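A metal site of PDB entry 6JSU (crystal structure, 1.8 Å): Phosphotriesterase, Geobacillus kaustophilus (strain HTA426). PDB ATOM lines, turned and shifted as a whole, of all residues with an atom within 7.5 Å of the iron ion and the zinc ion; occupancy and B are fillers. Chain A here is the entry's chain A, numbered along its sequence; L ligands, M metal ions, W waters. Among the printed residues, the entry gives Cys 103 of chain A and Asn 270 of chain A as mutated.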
ATOM      1  N   HIS A  27       0.757 -12.948 -28.286  1.00  0.00           N
ATOM      2  CA  HIS A  27       1.016 -11.871 -27.311  1.00  0.00           C
ATOM      3  C   HIS A  27       1.683 -10.675 -28.010  1.00  0.00           C
ATOM      4  O   HIS A  27       2.910 -10.622 -28.149  1.00  0.00           O
ATOM      5  CB  HIS A  27       1.869 -12.397 -26.134  1.00  0.00           C
ATOM      6  CG  HIS A  27       1.824 -11.521 -24.901  1.00  0.00           C
ATOM      7  ND1 HIS A  27       1.460 -12.023 -23.667  1.00  0.00           N
ATOM      8  CD2 HIS A  27       2.049 -10.201 -24.727  1.00  0.00           C
ATOM      9  CE1 HIS A  27       1.475 -11.052 -22.774  1.00  0.00           C
ATOM     10  NE2 HIS A  27       1.849  -9.945 -23.385  1.00  0.00           N
ATOM     11  N   GLU A  28       0.859  -9.717 -28.455  1.00  0.00           N
ATOM     12  CA  GLU A  28       1.326  -8.447 -28.999  1.00  0.00           C
ATOM     13  C   GLU A  28       0.395  -7.326 -28.550  1.00  0.00           C
ATOM     14  O   GLU A  28      -0.805  -7.530 -28.384  1.00  0.00           O
ATOM     15  CB  GLU A  28       1.420  -8.445 -30.556  1.00  0.00           C
ATOM     16  CG  GLU A  28       2.055  -9.659 -31.184  1.00  0.00           C
ATOM     17  CD  GLU A  28       3.577  -9.721 -31.023  1.00  0.00           C
ATOM     18  OE1 GLU A  28       4.201  -8.663 -30.829  1.00  0.00           O
ATOM     19  OE2 GLU A  28       4.153 -10.839 -31.103  1.00  0.00           O
ATOM     20  N   HIS A  29       0.959  -6.135 -28.336  1.00  0.00           N
ATOM     21  CA  HIS A  29       0.181  -4.961 -27.934  1.00  0.00           C
ATOM     22  C   HIS A  29       0.124  -3.944 -29.071  1.00  0.00           C
ATOM     23  O   HIS A  29       1.165  -3.429 -29.498  1.00  0.00           O
ATOM     24  CB  HIS A  29       0.770  -4.311 -26.678  1.00  0.00           C
ATOM     25  CG  HIS A  29       0.871  -5.227 -25.499  1.00  0.00           C
ATOM     26  ND1 HIS A  29      -0.188  -5.445 -24.637  1.00  0.00           N
ATOM     27  CD2 HIS A  29       1.899  -5.981 -25.035  1.00  0.00           C
ATOM     28  CE1 HIS A  29       0.186  -6.299 -23.700  1.00  0.00           C
ATOM     29  NE2 HIS A  29       1.452  -6.628 -23.906  1.00  0.00           N
ATOM     30  N   PHE A  32      -0.250   0.465 -25.728  1.00  0.00           N
ATOM     31  CA  PHE A  32       0.080   0.150 -24.342  1.00  0.00           C
ATOM     32  C   PHE A  32       0.522   1.420 -23.645  1.00  0.00           C
ATOM     33  O   PHE A  32       1.228   2.241 -24.233  1.00  0.00           O
ATOM     34  CB  PHE A  32       1.197  -0.896 -24.242  1.00  0.00           C
ATOM     35  CG  PHE A  32       1.553  -1.246 -22.809  1.00  0.00           C
ATOM     36  CD1 PHE A  32       0.877  -2.253 -22.137  1.00  0.00           C
ATOM     37  CD2 PHE A  32       2.555  -0.557 -22.136  1.00  0.00           C
ATOM     38  CE1 PHE A  32       1.189  -2.569 -20.828  1.00  0.00           C
ATOM     39  CE2 PHE A  32       2.871  -0.867 -20.839  1.00  0.00           C
ATOM     40  CZ  PHE A  32       2.189  -1.867 -20.182  1.00  0.00           C
ATOM     41  N   ASP A  72      -4.209  -9.732 -28.172  1.00  0.00           N
ATOM     42  CA  ASP A  72      -3.685  -8.508 -27.578  1.00  0.00           C
ATOM     43  C   ASP A  72      -4.135  -8.462 -26.119  1.00  0.00           C
ATOM     44  O   ASP A  72      -5.285  -8.100 -25.827  1.00  0.00           O
ATOM     45  CB  ASP A  72      -4.179  -7.284 -28.356  1.00  0.00           C
ATOM     46  CG  ASP A  72      -3.622  -5.986 -27.807  1.00  0.00           C
ATOM     47  OD1 ASP A  72      -3.368  -5.907 -26.598  1.00  0.00           O
ATOM     48  OD2 ASP A  72      -3.435  -5.026 -28.576  1.00  0.00           O
ATOM     49  N   PRO A  73      -3.276  -8.810 -25.180  1.00  0.00           N
ATOM     50  CA  PRO A  73      -3.731  -8.947 -23.782  1.00  0.00           C
ATOM     51  C   PRO A  73      -3.458  -7.709 -22.929  1.00  0.00           C
ATOM     52  O   PRO A  73      -3.223  -7.833 -21.722  1.00  0.00           O
ATOM     53  CB  PRO A  73      -2.919 -10.138 -23.295  1.00  0.00           C
ATOM     54  CG  PRO A  73      -1.588  -9.951 -23.977  1.00  0.00           C
ATOM     55  CD  PRO A  73      -1.895  -9.295 -25.338  1.00  0.00           C
ATOM     56  N   THR A  74      -3.492  -6.529 -23.546  1.00  0.00           N
ATOM     57  CA  THR A  74      -3.257  -5.281 -22.819  1.00  0.00           C
ATOM     58  C   THR A  74      -4.170  -5.171 -21.593  1.00  0.00           C
ATOM     59  O   THR A  74      -5.402  -5.190 -21.736  1.00  0.00           O
ATOM     60  CB  THR A  74      -3.482  -4.077 -23.733  1.00  0.00           C
ATOM     61  OG1 THR A  74      -2.587  -4.175 -24.847  1.00  0.00           O
ATOM     62  CG2 THR A  74      -3.198  -2.767 -22.981  1.00  0.00           C
ATOM     63  N   PRO A  75      -3.607  -5.054 -20.387  1.00  0.00           N
ATOM     64  CA  PRO A  75      -4.435  -5.049 -19.177  1.00  0.00           C
ATOM     65  C   PRO A  75      -5.353  -3.830 -19.096  1.00  0.00           C
ATOM     66  O   PRO A  75      -5.108  -2.796 -19.704  1.00  0.00           O
ATOM     67  CB  PRO A  75      -3.399  -5.016 -18.041  1.00  0.00           C
ATOM     68  CG  PRO A  75      -2.196  -5.694 -18.639  1.00  0.00           C
ATOM     69  CD  PRO A  75      -2.176  -5.239 -20.083  1.00  0.00           C
ATOM     70  N   CYS A 103      -2.841  -5.560 -14.497  1.00  0.00           N
ATOM     71  CA  CYS A 103      -1.399  -5.739 -14.419  1.00  0.00           C
ATOM     72  C   CYS A 103      -0.975  -6.255 -13.034  1.00  0.00           C
ATOM     73  O   CYS A 103      -1.738  -6.239 -12.058  1.00  0.00           O
ATOM     74  CB  CYS A 103      -0.720  -4.405 -14.740  1.00  0.00           C
ATOM     75  SG  CYS A 103       1.069  -4.463 -14.961  1.00  0.00           S
ATOM     76  N   TYR A 104       0.288  -6.685 -12.935  1.00  0.00           N
ATOM     77  CA  TYR A 104       0.788  -7.110 -11.640  1.00  0.00           C
ATOM     78  C   TYR A 104       1.040  -5.887 -10.752  1.00  0.00           C
ATOM     79  O   TYR A 104       1.147  -4.747 -11.221  1.00  0.00           O
ATOM     80  CB  TYR A 104       2.070  -7.948 -11.762  1.00  0.00           C
ATOM     81  CG  TYR A 104       3.286  -7.221 -12.293  1.00  0.00           C
ATOM     82  CD1 TYR A 104       3.418  -6.950 -13.647  1.00  0.00           C
ATOM     83  CD2 TYR A 104       4.300  -6.821 -11.436  1.00  0.00           C
ATOM     84  CE1 TYR A 104       4.539  -6.291 -14.131  1.00  0.00           C
ATOM     85  CE2 TYR A 104       5.415  -6.176 -11.904  1.00  0.00           C
ATOM     86  CZ  TYR A 104       5.534  -5.909 -13.247  1.00  0.00           C
ATOM     87  OH  TYR A 104       6.652  -5.255 -13.719  1.00  0.00           O
ATOM     88  N   KCX A 149      -6.543 -12.023 -18.558  1.00  0.00           N
ATOM     89  CA  KCX A 149      -5.133 -11.736 -18.357  1.00  0.00           C
ATOM     90  CB  KCX A 149      -4.764 -10.396 -19.024  1.00  0.00           C
ATOM     91  CG  KCX A 149      -3.320  -9.932 -18.758  1.00  0.00           C
ATOM     92  CD  KCX A 149      -2.316 -10.946 -19.314  1.00  0.00           C
ATOM     93  CE  KCX A 149      -0.886 -10.413 -19.236  1.00  0.00           C
ATOM     94  NZ  KCX A 149      -0.681  -9.306 -20.229  1.00  0.00           N
ATOM     95  C   KCX A 149      -4.790 -11.696 -16.878  1.00  0.00           C
ATOM     96  O   KCX A 149      -5.442 -11.007 -16.109  1.00  0.00           O
ATOM     97  CX  KCX A 149       0.560  -8.905 -20.518  1.00  0.00           C
ATOM     98  OQ1 KCX A 149       1.501  -9.460 -19.923  1.00  0.00           O
ATOM     99  OQ2 KCX A 149       0.777  -7.990 -21.332  1.00  0.00           O
ATOM    100  N   LEU A 150      -3.768 -12.439 -16.482  1.00  0.00           N
ATOM    101  CA  LEU A 150      -3.291 -12.433 -15.094  1.00  0.00           C
ATOM    102  C   LEU A 150      -1.809 -12.095 -15.066  1.00  0.00           C
ATOM    103  O   LEU A 150      -1.107 -12.299 -16.033  1.00  0.00           O
ATOM    104  CB  LEU A 150      -3.507 -13.798 -14.445  1.00  0.00           C
ATOM    105  CG  LEU A 150      -4.931 -14.279 -14.210  1.00  0.00           C
ATOM    106  CD1 LEU A 150      -4.854 -15.721 -13.716  1.00  0.00           C
ATOM    107  CD2 LEU A 150      -5.635 -13.368 -13.187  1.00  0.00           C
ATOM    108  N   ALA A 151      -1.315 -11.613 -13.929  1.00  0.00           N
ATOM    109  CA  ALA A 151       0.094 -11.224 -13.842  1.00  0.00           C
ATOM    110  C   ALA A 151       0.578 -11.345 -12.406  1.00  0.00           C
ATOM    111  O   ALA A 151      -0.173 -11.050 -11.468  1.00  0.00           O
ATOM    112  CB  ALA A 151       0.296  -9.790 -14.336  1.00  0.00           C
ATOM    113  N   THR A 181      -1.116 -15.437 -18.925  1.00  0.00           N
ATOM    114  CA  THR A 181      -0.444 -14.798 -17.796  1.00  0.00           C
ATOM    115  C   THR A 181       0.833 -14.066 -18.205  1.00  0.00           C
ATOM    116  O   THR A 181       1.409 -14.313 -19.265  1.00  0.00           O
ATOM    117  CB  THR A 181      -0.088 -15.795 -16.689  1.00  0.00           C
ATOM    118  OG1 THR A 181       1.149 -16.458 -16.999  1.00  0.00           O
ATOM    119  CG2 THR A 181      -1.203 -16.810 -16.468  1.00  0.00           C
ATOM    120  N   HIS A 182       1.222 -13.154 -17.326  1.00  0.00           N
ATOM    121  CA  HIS A 182       2.507 -12.476 -17.317  1.00  0.00           C
ATOM    122  C   HIS A 182       3.303 -13.017 -16.130  1.00  0.00           C
ATOM    123  O   HIS A 182       2.796 -13.039 -15.006  1.00  0.00           O
ATOM    124  CB  HIS A 182       2.261 -10.961 -17.191  1.00  0.00           C
ATOM    125  CG  HIS A 182       3.473 -10.149 -16.853  1.00  0.00           C
ATOM    126  ND1 HIS A 182       3.966  -9.177 -17.702  1.00  0.00           N
ATOM    127  CD2 HIS A 182       4.217 -10.073 -15.721  1.00  0.00           C
ATOM    128  CE1 HIS A 182       5.008  -8.591 -17.137  1.00  0.00           C
ATOM    129  NE2 HIS A 182       5.184  -9.115 -15.935  1.00  0.00           N
ATOM    130  N   THR A 183       4.541 -13.460 -16.372  1.00  0.00           N
ATOM    131  CA  THR A 183       5.498 -13.708 -15.289  1.00  0.00           C
ATOM    132  C   THR A 183       6.585 -12.626 -15.334  1.00  0.00           C
ATOM    133  O   THR A 183       6.972 -12.173 -16.407  1.00  0.00           O
ATOM    134  CB  THR A 183       6.172 -15.098 -15.353  1.00  0.00           C
ATOM    135  OG1 THR A 183       6.920 -15.264 -16.586  1.00  0.00           O
ATOM    136  CG2 THR A 183       5.129 -16.214 -15.184  1.00  0.00           C
ATOM    137  N   GLN A 184       7.056 -12.223 -14.159  1.00  0.00           N
ATOM    138  CA  GLN A 184       8.044 -11.164 -14.034  1.00  0.00           C
ATOM    139  C   GLN A 184       9.445 -11.766 -13.856  1.00  0.00           C
ATOM    140  O   GLN A 184       9.688 -12.555 -12.924  1.00  0.00           O
ATOM    141  CB  GLN A 184       7.674 -10.255 -12.857  1.00  0.00           C
ATOM    142  CG  GLN A 184       8.521  -9.009 -12.709  1.00  0.00           C
ATOM    143  CD  GLN A 184       8.360  -8.000 -13.855  1.00  0.00           C
ATOM    144  OE1 GLN A 184       7.468  -8.106 -14.713  1.00  0.00           O
ATOM    145  NE2 GLN A 184       9.236  -7.000 -13.859  1.00  0.00           N
ATOM    146  N   GLY A 209       2.854 -16.973 -19.514  1.00  0.00           N
ATOM    147  CA  GLY A 209       3.596 -16.094 -20.409  1.00  0.00           C
ATOM    148  C   GLY A 209       4.981 -15.703 -19.896  1.00  0.00           C
ATOM    149  O   GLY A 209       5.329 -15.931 -18.745  1.00  0.00           O
ATOM    150  N   HIS A 210       5.746 -15.087 -20.809  1.00  0.00           N
ATOM    151  CA  HIS A 210       7.124 -14.633 -20.588  1.00  0.00           C
ATOM    152  C   HIS A 210       8.021 -15.708 -19.985  1.00  0.00           C
ATOM    153  O   HIS A 210       8.916 -15.422 -19.173  1.00  0.00           O
ATOM    154  CB  HIS A 210       7.172 -13.362 -19.718  1.00  0.00           C
ATOM    155  CG  HIS A 210       6.165 -12.321 -20.094  1.00  0.00           C
ATOM    156  ND1 HIS A 210       5.768 -12.111 -21.394  1.00  0.00           N
ATOM    157  CD2 HIS A 210       5.488 -11.414 -19.345  1.00  0.00           C
ATOM    158  CE1 HIS A 210       4.885 -11.125 -21.426  1.00  0.00           C
ATOM    159  NE2 HIS A 210       4.689 -10.690 -20.193  1.00  0.00           N
ATOM    160  N   ASP A 233       7.460 -15.331 -25.495  1.00  0.00           N
ATOM    161  CA  ASP A 233       6.654 -14.288 -26.119  1.00  0.00           C
ATOM    162  C   ASP A 233       7.321 -12.926 -26.055  1.00  0.00           C
ATOM    163  O   ASP A 233       6.655 -11.911 -26.279  1.00  0.00           O
ATOM    164  CB  ASP A 233       5.254 -14.245 -25.487  1.00  0.00           C
ATOM    165  CG  ASP A 233       5.304 -14.080 -23.967  1.00  0.00           C
ATOM    166  OD1 ASP A 233       6.335 -13.611 -23.466  1.00  0.00           O
ATOM    167  OD2 ASP A 233       4.292 -14.402 -23.308  1.00  0.00           O
ATOM    168  N   ARG A 234       8.634 -12.868 -25.801  1.00  0.00           N
ATOM    169  CA  ARG A 234       9.345 -11.592 -25.732  1.00  0.00           C
ATOM    170  C   ARG A 234      10.562 -11.567 -26.655  1.00  0.00           C
ATOM    171  O   ARG A 234      11.574 -10.919 -26.374  1.00  0.00           O
ATOM    172  CB  ARG A 234       9.760 -11.275 -24.284  1.00  0.00           C
ATOM    173  CG  ARG A 234       8.600 -10.828 -23.435  1.00  0.00           C
ATOM    174  CD  ARG A 234       9.033 -10.435 -22.003  1.00  0.00           C
ATOM    175  NE  ARG A 234       8.180  -9.377 -21.490  1.00  0.00           N
ATOM    176  CZ  ARG A 234       8.204  -8.957 -20.228  1.00  0.00           C
ATOM    177  NH1 ARG A 234       9.046  -9.516 -19.374  1.00  0.00           N
ATOM    178  NH2 ARG A 234       7.377  -7.980 -19.833  1.00  0.00           N
ATOM    179  N   HIS A 269       6.310 -11.706 -29.664  1.00  0.00           N
ATOM    180  CA  HIS A 269       7.289 -10.635 -29.415  1.00  0.00           C
ATOM    181  C   HIS A 269       6.942  -9.724 -28.247  1.00  0.00           C
ATOM    182  O   HIS A 269       7.834  -9.050 -27.731  1.00  0.00           O
ATOM    183  CB  HIS A 269       7.448  -9.688 -30.622  1.00  0.00           C
ATOM    184  CG  HIS A 269       7.650 -10.370 -31.933  1.00  0.00           C
ATOM    185  ND1 HIS A 269       6.596 -10.762 -32.733  1.00  0.00           N
ATOM    186  CD2 HIS A 269       8.778 -10.639 -32.637  1.00  0.00           C
ATOM    187  CE1 HIS A 269       7.067 -11.278 -33.864  1.00  0.00           C
ATOM    188  NE2 HIS A 269       8.390 -11.211 -33.827  1.00  0.00           N
ATOM    189  N   ASN A 270       5.659  -9.635 -27.867  1.00  0.00           N
ATOM    190  CA  ASN A 270       5.199  -8.667 -26.872  1.00  0.00           C
ATOM    191  C   ASN A 270       5.487  -7.231 -27.325  1.00  0.00           C
ATOM    192  O   ASN A 270       5.824  -6.371 -26.507  1.00  0.00           O
ATOM    193  CB  ASN A 270       5.815  -8.950 -25.489  1.00  0.00           C
ATOM    194  CG  ASN A 270       5.152  -8.156 -24.365  1.00  0.00           C
ATOM    195  OD1 ASN A 270       3.940  -7.943 -24.356  1.00  0.00           O
ATOM    196  ND2 ASN A 270       5.967  -7.718 -23.392  1.00  0.00           N
ATOM    197  N   THR A 271       5.361  -6.963 -28.630  1.00  0.00           N
ATOM    198  CA  THR A 271       5.617  -5.601 -29.102  1.00  0.00           C
ATOM    199  C   THR A 271       4.635  -4.623 -28.476  1.00  0.00           C
ATOM    200  O   THR A 271       3.546  -4.980 -28.005  1.00  0.00           O
ATOM    201  CB  THR A 271       5.512  -5.484 -30.637  1.00  0.00           C
ATOM    202  OG1 THR A 271       4.257  -5.994 -31.081  1.00  0.00           O
ATOM    203  CG2 THR A 271       6.653  -6.201 -31.333  1.00  0.00           C
ATOM    204  N   VAL A 272       5.048  -3.368 -28.441  1.00  0.00           N
ATOM    205  CA  VAL A 272       4.164  -2.248 -28.148  1.00  0.00           C
ATOM    206  C   VAL A 272       4.266  -1.331 -29.360  1.00  0.00           C
ATOM    207  O   VAL A 272       5.288  -0.656 -29.559  1.00  0.00           O
ATOM    208  CB  VAL A 272       4.545  -1.519 -26.857  1.00  0.00           C
ATOM    209  CG1 VAL A 272       3.775  -0.210 -26.751  1.00  0.00           C
ATOM    210  CG2 VAL A 272       4.276  -2.431 -25.632  1.00  0.00           C
HETATM  211  O1  LIG L   1       3.866  -7.823 -21.330  1.00  0.00           O
HETATM  212 FE    FE M   1       2.343  -7.972 -22.763  1.00  0.00          FE
HETATM  213 ZN    ZN M   2       3.438  -9.087 -19.732  1.00  0.00          ZN
HETATM  214  O   HOH W   1       2.460  -6.624 -18.846  1.00  0.00           O
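The side-chain hydroxyl (OG1) of Thr 74 sits at hydrogen-bond distance from a ring nitrogen (ND1) of His 29 (2.7 Å).
The backbone NH of His 29 is in hydrogen-bond range of the backbone carbonyl oxygen of Thr 271.
The side-chain hydroxyl (OG1) of Thr 183 sits at hydrogen-bond distance from the backbone carbonyl oxygen (O) of His 210 (3.3 Å).
The side-chain carboxylate of Asp 233 lies within hydrogen-bond range of a ring nitrogen (ND1) of His 210, at 2.6 Å.
NE2 of His 182 lies within hydrogen-bond range of OE1 of Gln 184 (2.8 Å).
N of His 182 lies within hydrogen-bond range of O of Leu 150, 2.8 Å away.
The backbone NH of Asn 270 sits at hydrogen-bond distance from the side-chain carboxylate of Glu 28, 3.4 Å away.
The backbone NH (N) of Asn 270 sits at hydrogen-bond distance from the backbone carbonyl oxygen (O) of Asp 233, 2.9 Å away.
Within 4 Å of the iron ion: His 27, His 29, KCX 149 and Asn 270.
The iron ion is bound by NE2 of His 29, at 2.0 Å.
O1 of the ligand binds the iron ion (2.1 Å).
OQ2 of KCX 149 binds the iron ion (2.1 Å).
A ring nitrogen (NE2) of His 27 binds the iron ion.
The iron ion is bound by OD1 of Asn 270 (2.3 Å).
The zinc ion is bound by OQ1 of KCX 149 (2.0 Å), O1 of the ligand (2.1 Å), NE2 of His 210 (2.1 Å) and ND1 of His 182 (2.1 Å).
The zinc ion has four donor atoms within binding distance.
Slightly farther from the zinc ion lies water W1 (2.8 Å).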
